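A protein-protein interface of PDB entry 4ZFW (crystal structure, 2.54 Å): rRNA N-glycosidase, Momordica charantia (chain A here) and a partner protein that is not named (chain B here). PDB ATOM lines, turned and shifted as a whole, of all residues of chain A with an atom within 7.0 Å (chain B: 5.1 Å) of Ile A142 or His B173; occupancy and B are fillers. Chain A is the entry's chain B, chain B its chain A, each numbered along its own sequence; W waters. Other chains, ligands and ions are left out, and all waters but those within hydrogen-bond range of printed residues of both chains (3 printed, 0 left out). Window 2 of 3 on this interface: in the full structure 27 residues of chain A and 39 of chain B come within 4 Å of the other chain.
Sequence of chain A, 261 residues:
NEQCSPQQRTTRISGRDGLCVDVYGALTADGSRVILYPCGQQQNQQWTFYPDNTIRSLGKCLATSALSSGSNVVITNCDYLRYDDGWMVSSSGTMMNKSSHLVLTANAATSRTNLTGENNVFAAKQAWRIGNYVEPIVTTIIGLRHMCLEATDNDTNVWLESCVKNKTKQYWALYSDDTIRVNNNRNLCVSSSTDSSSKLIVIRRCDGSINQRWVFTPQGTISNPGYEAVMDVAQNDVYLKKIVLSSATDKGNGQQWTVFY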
ATOM      1  N   THR A 139       9.096 -13.753   5.222  1.00  0.00           N
ATOM      2  CA  THR A 139       9.907 -12.928   6.089  1.00  0.00           C
ATOM      3  C   THR A 139      11.339 -12.791   5.579  1.00  0.00           C
ATOM      4  O   THR A 139      11.767 -13.576   4.737  1.00  0.00           O
ATOM      5  CB  THR A 139       9.873 -13.495   7.531  1.00  0.00           C
ATOM      6  OG1 THR A 139      10.466 -12.566   8.431  1.00  0.00           O
ATOM      7  CG2 THR A 139      10.626 -14.771   7.629  1.00  0.00           C
ATOM      8  N   THR A 140      12.039 -11.745   6.038  1.00  0.00           N
ATOM      9  CA  THR A 140      13.501 -11.707   5.979  1.00  0.00           C
ATOM     10  C   THR A 140      14.004 -12.087   7.349  1.00  0.00           C
ATOM     11  O   THR A 140      13.303 -11.939   8.333  1.00  0.00           O
ATOM     12  CB  THR A 140      14.085 -10.354   5.543  1.00  0.00           C
ATOM     13  OG1 THR A 140      13.784  -9.315   6.495  1.00  0.00           O
ATOM     14  CG2 THR A 140      13.561  -9.975   4.171  1.00  0.00           C
ATOM     15  N   ILE A 141      15.200 -12.639   7.403  1.00  0.00           N
ATOM     16  CA  ILE A 141      15.776 -13.090   8.654  1.00  0.00           C
ATOM     17  C   ILE A 141      17.088 -12.385   8.830  1.00  0.00           C
ATOM     18  O   ILE A 141      18.004 -12.552   8.037  1.00  0.00           O
ATOM     19  CB  ILE A 141      15.943 -14.601   8.653  1.00  0.00           C
ATOM     20  CG1 ILE A 141      14.552 -15.222   8.634  1.00  0.00           C
ATOM     21  CG2 ILE A 141      16.712 -15.067   9.880  1.00  0.00           C
ATOM     22  CD1 ILE A 141      14.555 -16.702   8.459  1.00  0.00           C
ATOM     23  N   ILE A 142      17.146 -11.581   9.881  1.00  0.00           N
ATOM     24  CA  ILE A 142      18.211 -10.618  10.090  1.00  0.00           C
ATOM     25  C   ILE A 142      19.084 -11.078  11.233  1.00  0.00           C
ATOM     26  O   ILE A 142      18.611 -11.366  12.337  1.00  0.00           O
ATOM     27  CB  ILE A 142      17.632  -9.215  10.358  1.00  0.00           C
ATOM     28  CG1 ILE A 142      16.868  -8.746   9.110  1.00  0.00           C
ATOM     29  CG2 ILE A 142      18.738  -8.200  10.672  1.00  0.00           C
ATOM     30  CD1 ILE A 142      15.891  -7.613   9.372  1.00  0.00           C
ATOM     31  N   GLY A 143      20.373 -11.133  10.939  1.00  0.00           N
ATOM     32  CA  GLY A 143      21.373 -11.480  11.922  1.00  0.00           C
ATOM     33  C   GLY A 143      22.469 -10.446  12.077  1.00  0.00           C
ATOM     34  O   GLY A 143      22.210  -9.226  12.073  1.00  0.00           O
ATOM     35  N   LEU A 144      23.690 -10.977  12.226  1.00  0.00           N
ATOM     36  CA  LEU A 144      24.873 -10.242  12.621  1.00  0.00           C
ATOM     37  C   LEU A 144      25.188  -9.129  11.632  1.00  0.00           C
ATOM     38  O   LEU A 144      24.995  -9.283  10.418  1.00  0.00           O
ATOM     39  CB  LEU A 144      26.059 -11.220  12.709  1.00  0.00           C
ATOM     40  CG  LEU A 144      27.332 -10.754  13.415  1.00  0.00           C
ATOM     41  CD1 LEU A 144      27.047 -10.443  14.889  1.00  0.00           C
ATOM     42  CD2 LEU A 144      28.426 -11.799  13.249  1.00  0.00           C
ATOM     43  N   ARG A 145      25.670  -8.010  12.163  1.00  0.00           N
ATOM     44  CA  ARG A 145      25.928  -6.795  11.374  1.00  0.00           C
ATOM     45  C   ARG A 145      24.712  -6.277  10.568  1.00  0.00           C
ATOM     46  O   ARG A 145      24.872  -5.487   9.637  1.00  0.00           O
ATOM     47  CB  ARG A 145      27.184  -6.976  10.503  1.00  0.00           C
ATOM     48  CG  ARG A 145      28.456  -6.963  11.349  1.00  0.00           C
ATOM     49  CD  ARG A 145      29.719  -7.128  10.524  1.00  0.00           C
ATOM     50  NE  ARG A 145      29.876  -6.055   9.540  1.00  0.00           N
ATOM     51  CZ  ARG A 145      30.437  -4.869   9.770  1.00  0.00           C
ATOM     52  NH1 ARG A 145      30.938  -4.542  10.963  1.00  0.00           N
ATOM     53  NH2 ARG A 145      30.487  -3.986   8.782  1.00  0.00           N
ATOM     54  N   HIS A 146      23.510  -6.651  11.019  1.00  0.00           N
ATOM     55  CA  HIS A 146      22.230  -6.240  10.441  1.00  0.00           C
ATOM     56  C   HIS A 146      22.069  -6.679   9.011  1.00  0.00           C
ATOM     57  O   HIS A 146      21.440  -5.985   8.202  1.00  0.00           O
ATOM     58  CB  HIS A 146      22.012  -4.719  10.528  1.00  0.00           C
ATOM     59  CG  HIS A 146      22.587  -4.102  11.748  1.00  0.00           C
ATOM     60  ND1 HIS A 146      21.904  -4.035  12.937  1.00  0.00           N
ATOM     61  CD2 HIS A 146      23.789  -3.516  11.961  1.00  0.00           C
ATOM     62  CE1 HIS A 146      22.661  -3.425  13.832  1.00  0.00           C
ATOM     63  NE2 HIS A 146      23.814  -3.110  13.268  1.00  0.00           N
ATOM     64  N   MET A 147      22.626  -7.833   8.709  1.00  0.00           N
ATOM     65  CA  MET A 147      22.584  -8.377   7.358  1.00  0.00           C
ATOM     66  C   MET A 147      21.524  -9.447   7.310  1.00  0.00           C
ATOM     67  O   MET A 147      21.098  -9.935   8.331  1.00  0.00           O
ATOM     68  CB  MET A 147      23.964  -8.927   6.990  1.00  0.00           C
ATOM     69  CG  MET A 147      25.037  -7.852   6.921  1.00  0.00           C
ATOM     70  SD  MET A 147      26.660  -8.566   6.600  1.00  0.00           S
ATOM     71  CE  MET A 147      26.621  -8.895   4.858  1.00  0.00           C
ATOM     72  N   CYS A 148      21.104  -9.800   6.109  1.00  0.00           N
ATOM     73  CA  CYS A 148      19.978 -10.721   5.870  1.00  0.00           C
ATOM     74  C   CYS A 148      20.505 -12.045   5.429  1.00  0.00           C
ATOM     75  O   CYS A 148      21.428 -12.083   4.633  1.00  0.00           O
ATOM     76  CB  CYS A 148      19.076 -10.164   4.757  1.00  0.00           C
ATOM     77  SG  CYS A 148      17.962  -8.841   5.320  1.00  0.00           S
ATOM     78  N   LEU A 149      19.929 -13.141   5.907  1.00  0.00           N
ATOM     79  CA  LEU A 149      20.194 -14.437   5.269  1.00  0.00           C
ATOM     80  C   LEU A 149      19.738 -14.392   3.812  1.00  0.00           C
ATOM     81  O   LEU A 149      18.630 -13.943   3.512  1.00  0.00           O
ATOM     82  CB  LEU A 149      19.466 -15.596   5.950  1.00  0.00           C
ATOM     83  CG  LEU A 149      19.971 -16.011   7.319  1.00  0.00           C
ATOM     84  CD1 LEU A 149      19.032 -17.059   7.858  1.00  0.00           C
ATOM     85  CD2 LEU A 149      21.395 -16.551   7.292  1.00  0.00           C
ATOM     86  N   LEU A 160      24.954 -14.640   5.188  1.00  0.00           N
ATOM     87  CA  LEU A 160      24.540 -13.268   5.332  1.00  0.00           C
ATOM     88  C   LEU A 160      25.027 -12.324   4.219  1.00  0.00           C
ATOM     89  O   LEU A 160      26.184 -12.407   3.758  1.00  0.00           O
ATOM     90  CB  LEU A 160      25.005 -12.748   6.673  1.00  0.00           C
ATOM     91  CG  LEU A 160      24.292 -13.415   7.859  1.00  0.00           C
ATOM     92  CD1 LEU A 160      25.143 -13.175   9.088  1.00  0.00           C
ATOM     93  CD2 LEU A 160      22.864 -12.904   8.108  1.00  0.00           C
ATOM     94  N   CYS A 163      21.141  -6.308   3.467  1.00  0.00           N
ATOM     95  CA  CYS A 163      19.709  -6.437   3.193  1.00  0.00           C
ATOM     96  C   CYS A 163      19.309  -5.549   2.019  1.00  0.00           C
ATOM     97  O   CYS A 163      19.725  -4.410   1.935  1.00  0.00           O
ATOM     98  CB  CYS A 163      18.883  -6.087   4.422  1.00  0.00           C
ATOM     99  SG  CYS A 163      19.153  -7.221   5.790  1.00  0.00           S
ATOM    100  N   GLY A 220      15.794 -14.742  21.097  1.00  0.00           N
ATOM    101  CA  GLY A 220      16.417 -14.193  19.912  1.00  0.00           C
ATOM    102  C   GLY A 220      17.264 -15.193  19.147  1.00  0.00           C
ATOM    103  O   GLY A 220      17.955 -14.800  18.208  1.00  0.00           O
ATOM    104  N   ILE A 222      17.680 -18.983  16.946  1.00  0.00           N
ATOM    105  CA  ILE A 222      17.015 -19.899  16.050  1.00  0.00           C
ATOM    106  C   ILE A 222      17.514 -21.314  16.375  1.00  0.00           C
ATOM    107  O   ILE A 222      18.656 -21.690  16.062  1.00  0.00           O
ATOM    108  CB  ILE A 222      17.304 -19.569  14.589  1.00  0.00           C
ATOM    109  CG1 ILE A 222      17.100 -18.079  14.343  1.00  0.00           C
ATOM    110  CG2 ILE A 222      16.365 -20.380  13.700  1.00  0.00           C
ATOM    111  CD1 ILE A 222      17.136 -17.634  12.875  1.00  0.00           C
ATOM    112  N   GLN A 256      22.260 -14.351  17.546  1.00  0.00           N
ATOM    113  CA  GLN A 256      21.073 -13.468  17.670  1.00  0.00           C
ATOM    114  C   GLN A 256      20.425 -13.117  16.342  1.00  0.00           C
ATOM    115  O   GLN A 256      21.069 -12.645  15.403  1.00  0.00           O
ATOM    116  CB  GLN A 256      21.428 -12.158  18.387  1.00  0.00           C
ATOM    117  CG  GLN A 256      21.552 -12.332  19.897  1.00  0.00           C
ATOM    118  CD  GLN A 256      20.210 -12.552  20.552  1.00  0.00           C
ATOM    119  OE1 GLN A 256      19.294 -11.722  20.439  1.00  0.00           O
ATOM    120  NE2 GLN A 256      20.064 -13.680  21.194  1.00  0.00           N
ATOM    121  N   TRP A 257      19.117 -13.299  16.284  1.00  0.00           N
ATOM    122  CA  TRP A 257      18.374 -13.159  15.044  1.00  0.00           C
ATOM    123  C   TRP A 257      17.058 -12.446  15.258  1.00  0.00           C
ATOM    124  O   TRP A 257      16.467 -12.500  16.336  1.00  0.00           O
ATOM    125  CB  TRP A 257      18.127 -14.537  14.435  1.00  0.00           C
ATOM    126  CG  TRP A 257      19.377 -15.342  14.234  1.00  0.00           C
ATOM    127  CD1 TRP A 257      19.950 -16.193  15.138  1.00  0.00           C
ATOM    128  CD2 TRP A 257      20.215 -15.375  13.063  1.00  0.00           C
ATOM    129  NE1 TRP A 257      21.088 -16.765  14.597  1.00  0.00           N
ATOM    130  CE2 TRP A 257      21.270 -16.276  13.326  1.00  0.00           C
ATOM    131  CE3 TRP A 257      20.180 -14.722  11.821  1.00  0.00           C
ATOM    132  CZ2 TRP A 257      22.284 -16.541  12.394  1.00  0.00           C
ATOM    133  CZ3 TRP A 257      21.191 -14.989  10.888  1.00  0.00           C
ATOM    134  CH2 TRP A 257      22.227 -15.896  11.181  1.00  0.00           C
ATOM    135  N   THR A 258      16.611 -11.799  14.191  1.00  0.00           N
ATOM    136  CA  THR A 258      15.346 -11.097  14.137  1.00  0.00           C
ATOM    137  C   THR A 258      14.566 -11.463  12.873  1.00  0.00           C
ATOM    138  O   THR A 258      15.103 -11.569  11.770  1.00  0.00           O
ATOM    139  CB  THR A 258      15.546  -9.581  14.080  1.00  0.00           C
ATOM    140  OG1 THR A 258      16.416  -9.164  15.117  1.00  0.00           O
ATOM    141  CG2 THR A 258      14.254  -8.830  14.256  1.00  0.00           C
ATOM    142  N   VAL A 259      13.268 -11.540  13.051  1.00  0.00           N
ATOM    143  CA  VAL A 259      12.333 -11.829  12.008  1.00  0.00           C
ATOM    144  C   VAL A 259      11.731 -10.524  11.544  1.00  0.00           C
ATOM    145  O   VAL A 259      11.127  -9.834  12.347  1.00  0.00           O
ATOM    146  CB  VAL A 259      11.230 -12.723  12.599  1.00  0.00           C
ATOM    147  CG1 VAL A 259      10.014 -12.821  11.697  1.00  0.00           C
ATOM    148  CG2 VAL A 259      11.820 -14.075  12.885  1.00  0.00           C
ATOM    149  N   PHE A 260      11.836 -10.217  10.253  1.00  0.00           N
ATOM    150  CA  PHE A 260      11.192  -9.027   9.691  1.00  0.00           C
ATOM    151  C   PHE A 260      10.233  -9.397   8.542  1.00  0.00           C
ATOM    152  O   PHE A 260      10.658  -9.960   7.545  1.00  0.00           O
ATOM    153  CB  PHE A 260      12.274  -8.068   9.242  1.00  0.00           C
ATOM    154  CG  PHE A 260      11.772  -6.713   8.955  1.00  0.00           C
ATOM    155  CD1 PHE A 260      11.500  -5.832   9.993  1.00  0.00           C
ATOM    156  CD2 PHE A 260      11.533  -6.311   7.639  1.00  0.00           C
ATOM    157  CE1 PHE A 260      10.998  -4.560   9.733  1.00  0.00           C
ATOM    158  CE2 PHE A 260      11.042  -5.031   7.373  1.00  0.00           C
ATOM    159  CZ  PHE A 260      10.781  -4.153   8.425  1.00  0.00           C
ATOM    160  N   GLN B 169      13.642  -2.905  14.550  1.00  0.00           N
ATOM    161  CA  GLN B 169      14.240  -3.146  13.255  1.00  0.00           C
ATOM    162  C   GLN B 169      13.867  -2.125  12.173  1.00  0.00           C
ATOM    163  O   GLN B 169      14.672  -1.830  11.283  1.00  0.00           O
ATOM    164  CB  GLN B 169      13.889  -4.568  12.799  1.00  0.00           C
ATOM    165  CG  GLN B 169      14.931  -5.203  11.891  1.00  0.00           C
ATOM    166  CD  GLN B 169      16.301  -5.256  12.530  1.00  0.00           C
ATOM    167  OE1 GLN B 169      16.489  -5.661  13.711  1.00  0.00           O
ATOM    168  NE2 GLN B 169      17.271  -4.840  11.760  1.00  0.00           N
ATOM    169  N   LYS B 170      12.646  -1.604  12.248  1.00  0.00           N
ATOM    170  CA  LYS B 170      12.251  -0.445  11.446  1.00  0.00           C
ATOM    171  C   LYS B 170      13.147   0.756  11.759  1.00  0.00           C
ATOM    172  O   LYS B 170      13.530   1.482  10.855  1.00  0.00           O
ATOM    173  CB  LYS B 170      10.808  -0.028  11.720  1.00  0.00           C
ATOM    174  CG  LYS B 170       9.750  -1.030  11.391  1.00  0.00           C
ATOM    175  CD  LYS B 170       9.587  -1.202   9.924  1.00  0.00           C
ATOM    176  CE  LYS B 170       8.947   0.010   9.256  1.00  0.00           C
ATOM    177  NZ  LYS B 170       8.568  -0.391   7.867  1.00  0.00           N
ATOM    178  N   VAL B 171      13.465   0.977  13.028  1.00  0.00           N
ATOM    179  CA  VAL B 171      14.354   2.077  13.378  1.00  0.00           C
ATOM    180  C   VAL B 171      15.796   1.809  12.896  1.00  0.00           C
ATOM    181  O   VAL B 171      16.511   2.728  12.523  1.00  0.00           O
ATOM    182  CB  VAL B 171      14.317   2.376  14.880  1.00  0.00           C
ATOM    183  CG1 VAL B 171      15.346   3.425  15.242  1.00  0.00           C
ATOM    184  CG2 VAL B 171      12.937   2.883  15.276  1.00  0.00           C
ATOM    185  N   ILE B 172      16.215   0.550  12.907  1.00  0.00           N
ATOM    186  CA  ILE B 172      17.522   0.194  12.394  1.00  0.00           C
ATOM    187  C   ILE B 172      17.562   0.411  10.891  1.00  0.00           C
ATOM    188  O   ILE B 172      18.494   1.053  10.387  1.00  0.00           O
ATOM    189  CB  ILE B 172      17.904  -1.250  12.790  1.00  0.00           C
ATOM    190  CG1 ILE B 172      18.128  -1.334  14.325  1.00  0.00           C
ATOM    191  CG2 ILE B 172      19.159  -1.684  12.067  1.00  0.00           C
ATOM    192  CD1 ILE B 172      17.868  -2.718  14.898  1.00  0.00           C
ATOM    193  N   HIS B 173      16.560  -0.104  10.192  1.00  0.00           N
ATOM    194  CA  HIS B 173      16.478   0.074   8.759  1.00  0.00           C
ATOM    195  C   HIS B 173      16.471   1.548   8.398  1.00  0.00           C
ATOM    196  O   HIS B 173      17.123   1.954   7.439  1.00  0.00           O
ATOM    197  CB  HIS B 173      15.235  -0.607   8.178  1.00  0.00           C
ATOM    198  CG  HIS B 173      15.348  -2.094   8.091  1.00  0.00           C
ATOM    199  ND1 HIS B 173      14.255  -2.914   7.944  1.00  0.00           N
ATOM    200  CD2 HIS B 173      16.422  -2.913   8.151  1.00  0.00           C
ATOM    201  CE1 HIS B 173      14.650  -4.176   7.887  1.00  0.00           C
ATOM    202  NE2 HIS B 173      15.964  -4.201   8.007  1.00  0.00           N
ATOM    203  N   SER B 174      15.761   2.355   9.188  1.00  0.00           N
ATOM    204  CA  SER B 174      15.835   3.801   9.029  1.00  0.00           C
ATOM    205  C   SER B 174      17.250   4.361   9.220  1.00  0.00           C
ATOM    206  O   SER B 174      17.665   5.201   8.440  1.00  0.00           O
ATOM    207  CB  SER B 174      14.866   4.500   9.961  1.00  0.00           C
ATOM    208  OG  SER B 174      15.166   5.868  10.066  1.00  0.00           O
ATOM    209  N   ILE B 175      17.980   3.922  10.242  1.00  0.00           N
ATOM    210  CA  ILE B 175      19.333   4.459  10.499  1.00  0.00           C
ATOM    211  C   ILE B 175      20.287   4.121   9.352  1.00  0.00           C
ATOM    212  O   ILE B 175      21.007   4.970   8.860  1.00  0.00           O
ATOM    213  CB  ILE B 175      19.919   3.958  11.835  1.00  0.00           C
ATOM    214  CG1 ILE B 175      19.112   4.520  13.023  1.00  0.00           C
ATOM    215  CG2 ILE B 175      21.362   4.394  11.993  1.00  0.00           C
ATOM    216  CD1 ILE B 175      19.170   3.664  14.270  1.00  0.00           C
ATOM    217  N   MET B 176      20.227   2.886   8.897  1.00  0.00           N
ATOM    218  CA  MET B 176      21.116   2.408   7.865  1.00  0.00           C
ATOM    219  C   MET B 176      20.773   2.914   6.477  1.00  0.00           C
ATOM    220  O   MET B 176      21.662   3.222   5.713  1.00  0.00           O
ATOM    221  CB  MET B 176      21.132   0.879   7.871  1.00  0.00           C
ATOM    222  CG  MET B 176      21.683   0.360   9.184  1.00  0.00           C
ATOM    223  SD  MET B 176      21.931  -1.402   9.199  1.00  0.00           S
ATOM    224  CE  MET B 176      23.388  -1.530   8.160  1.00  0.00           C
ATOM    225  N   ASP B 177      19.505   2.994   6.139  1.00  0.00           N
ATOM    226  CA  ASP B 177      19.128   3.526   4.846  1.00  0.00           C
ATOM    227  C   ASP B 177      19.261   5.048   4.794  1.00  0.00           C
ATOM    228  O   ASP B 177      19.224   5.604   3.703  1.00  0.00           O
ATOM    229  CB  ASP B 177      17.722   3.079   4.456  1.00  0.00           C
ATOM    230  CG  ASP B 177      17.607   1.551   4.314  1.00  0.00           C
ATOM    231  OD1 ASP B 177      18.665   0.901   4.160  1.00  0.00           O
ATOM    232  OD2 ASP B 177      16.471   0.990   4.366  1.00  0.00           O
ATOM    233  N   MET B 178      19.464   5.714   5.937  1.00  0.00           N
ATOM    234  CA  MET B 178      19.395   7.179   6.029  1.00  0.00           C
ATOM    235  C   MET B 178      18.007   7.640   5.474  1.00  0.00           C
ATOM    236  O   MET B 178      17.925   8.539   4.642  1.00  0.00           O
ATOM    237  CB  MET B 178      20.574   7.849   5.284  1.00  0.00           C
ATOM    238  CG  MET B 178      21.948   7.163   5.384  1.00  0.00           C
ATOM    239  SD  MET B 178      23.053   7.318   3.920  1.00  0.00           S
ATOM    240  CE  MET B 178      22.235   6.420   2.577  1.00  0.00           C
HETATM  241  O   HOH W   1      15.597  -6.160  16.378  1.00  0.00           O
HETATM  242  O   HOH W   2      18.912  -4.637   8.796  1.00  0.00           O
HETATM  243  O   HOH W   3      19.733  -6.190  13.256  1.00  0.00           O
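Printed residues of chain A that touch a printed residue of chain B: Ile A142, His A146, Thr A258 and Phe A260. Of the 10 printed residues of chain B, 5 touch a printed residue of chain A. Hydrophobic or aromatic side chains of chain B within 4 Å of the printed part of chain A: Ile B172, His B173 and Met B176. Among the printed residues, 8 pairs touch across the chains.
Among the printed residues, pairs that only touch across the chains: Phe A260 with Lys B170, His A146 with Met B176, Ile A142 with Gln B169, Ile A142 with His B173, His A146 with Ile B172, Phe A260 with His B173, Thr A258 with Gln B169 and Phe A260 with Gln B169.
The backbone carbonyl oxygen of Phe A260 is in hydrogen-bond range of the side-chain hydroxyl of Thr A139. The backbone carbonyl oxygen (O) of Phe A260 lies within hydrogen-bond range of the backbone NH (N) of Thr A140, 2.7 Å away. The backbone carbonyl oxygen (O) of Ile A142 sits at hydrogen-bond distance from the backbone NH (N) of Thr A258 (2.8 Å). The side-chain sulfur of Cys A163 is disulfide-bonded to the side-chain sulfur of Cys A148 (2.1 Å).
Water W1 lies within hydrogen-bond range of OE1 of Gln B169 (2.9 Å) and OG1 of Thr A258 (3.4 Å). Water W2 lies within hydrogen-bond range of O of His A146 (2.9 Å), NE2 of His B173 (3.1 Å) and NE2 of Gln B169 (3.4 Å). Water W3 bridges ND1 of His A146 (3.1 Å) and NE2 of Gln B169 (3.2 Å).
Gly A143 touches none of the printed residues of chain B. Arg A145 touches none of the printed residues of chain B. Of the printed residues of chain B, His A146 touches Ile B172 (3.7 Å) and Met B176 (3.6 Å). Of the printed residues of chain A, Gln B169 touches Ile A142 (3.6 Å), Thr A258 (3.8 Å) and Phe A260 (3.9 Å). His B173 touches just these residues of chain A: Ile A142 and Phe A260. The nearest residue of chain A that does not touch His B173 is Cys A163 (4.9 Å). The nearest printed residue of chain A that does not touch Met B176 is Arg A145 (4.5 Å).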
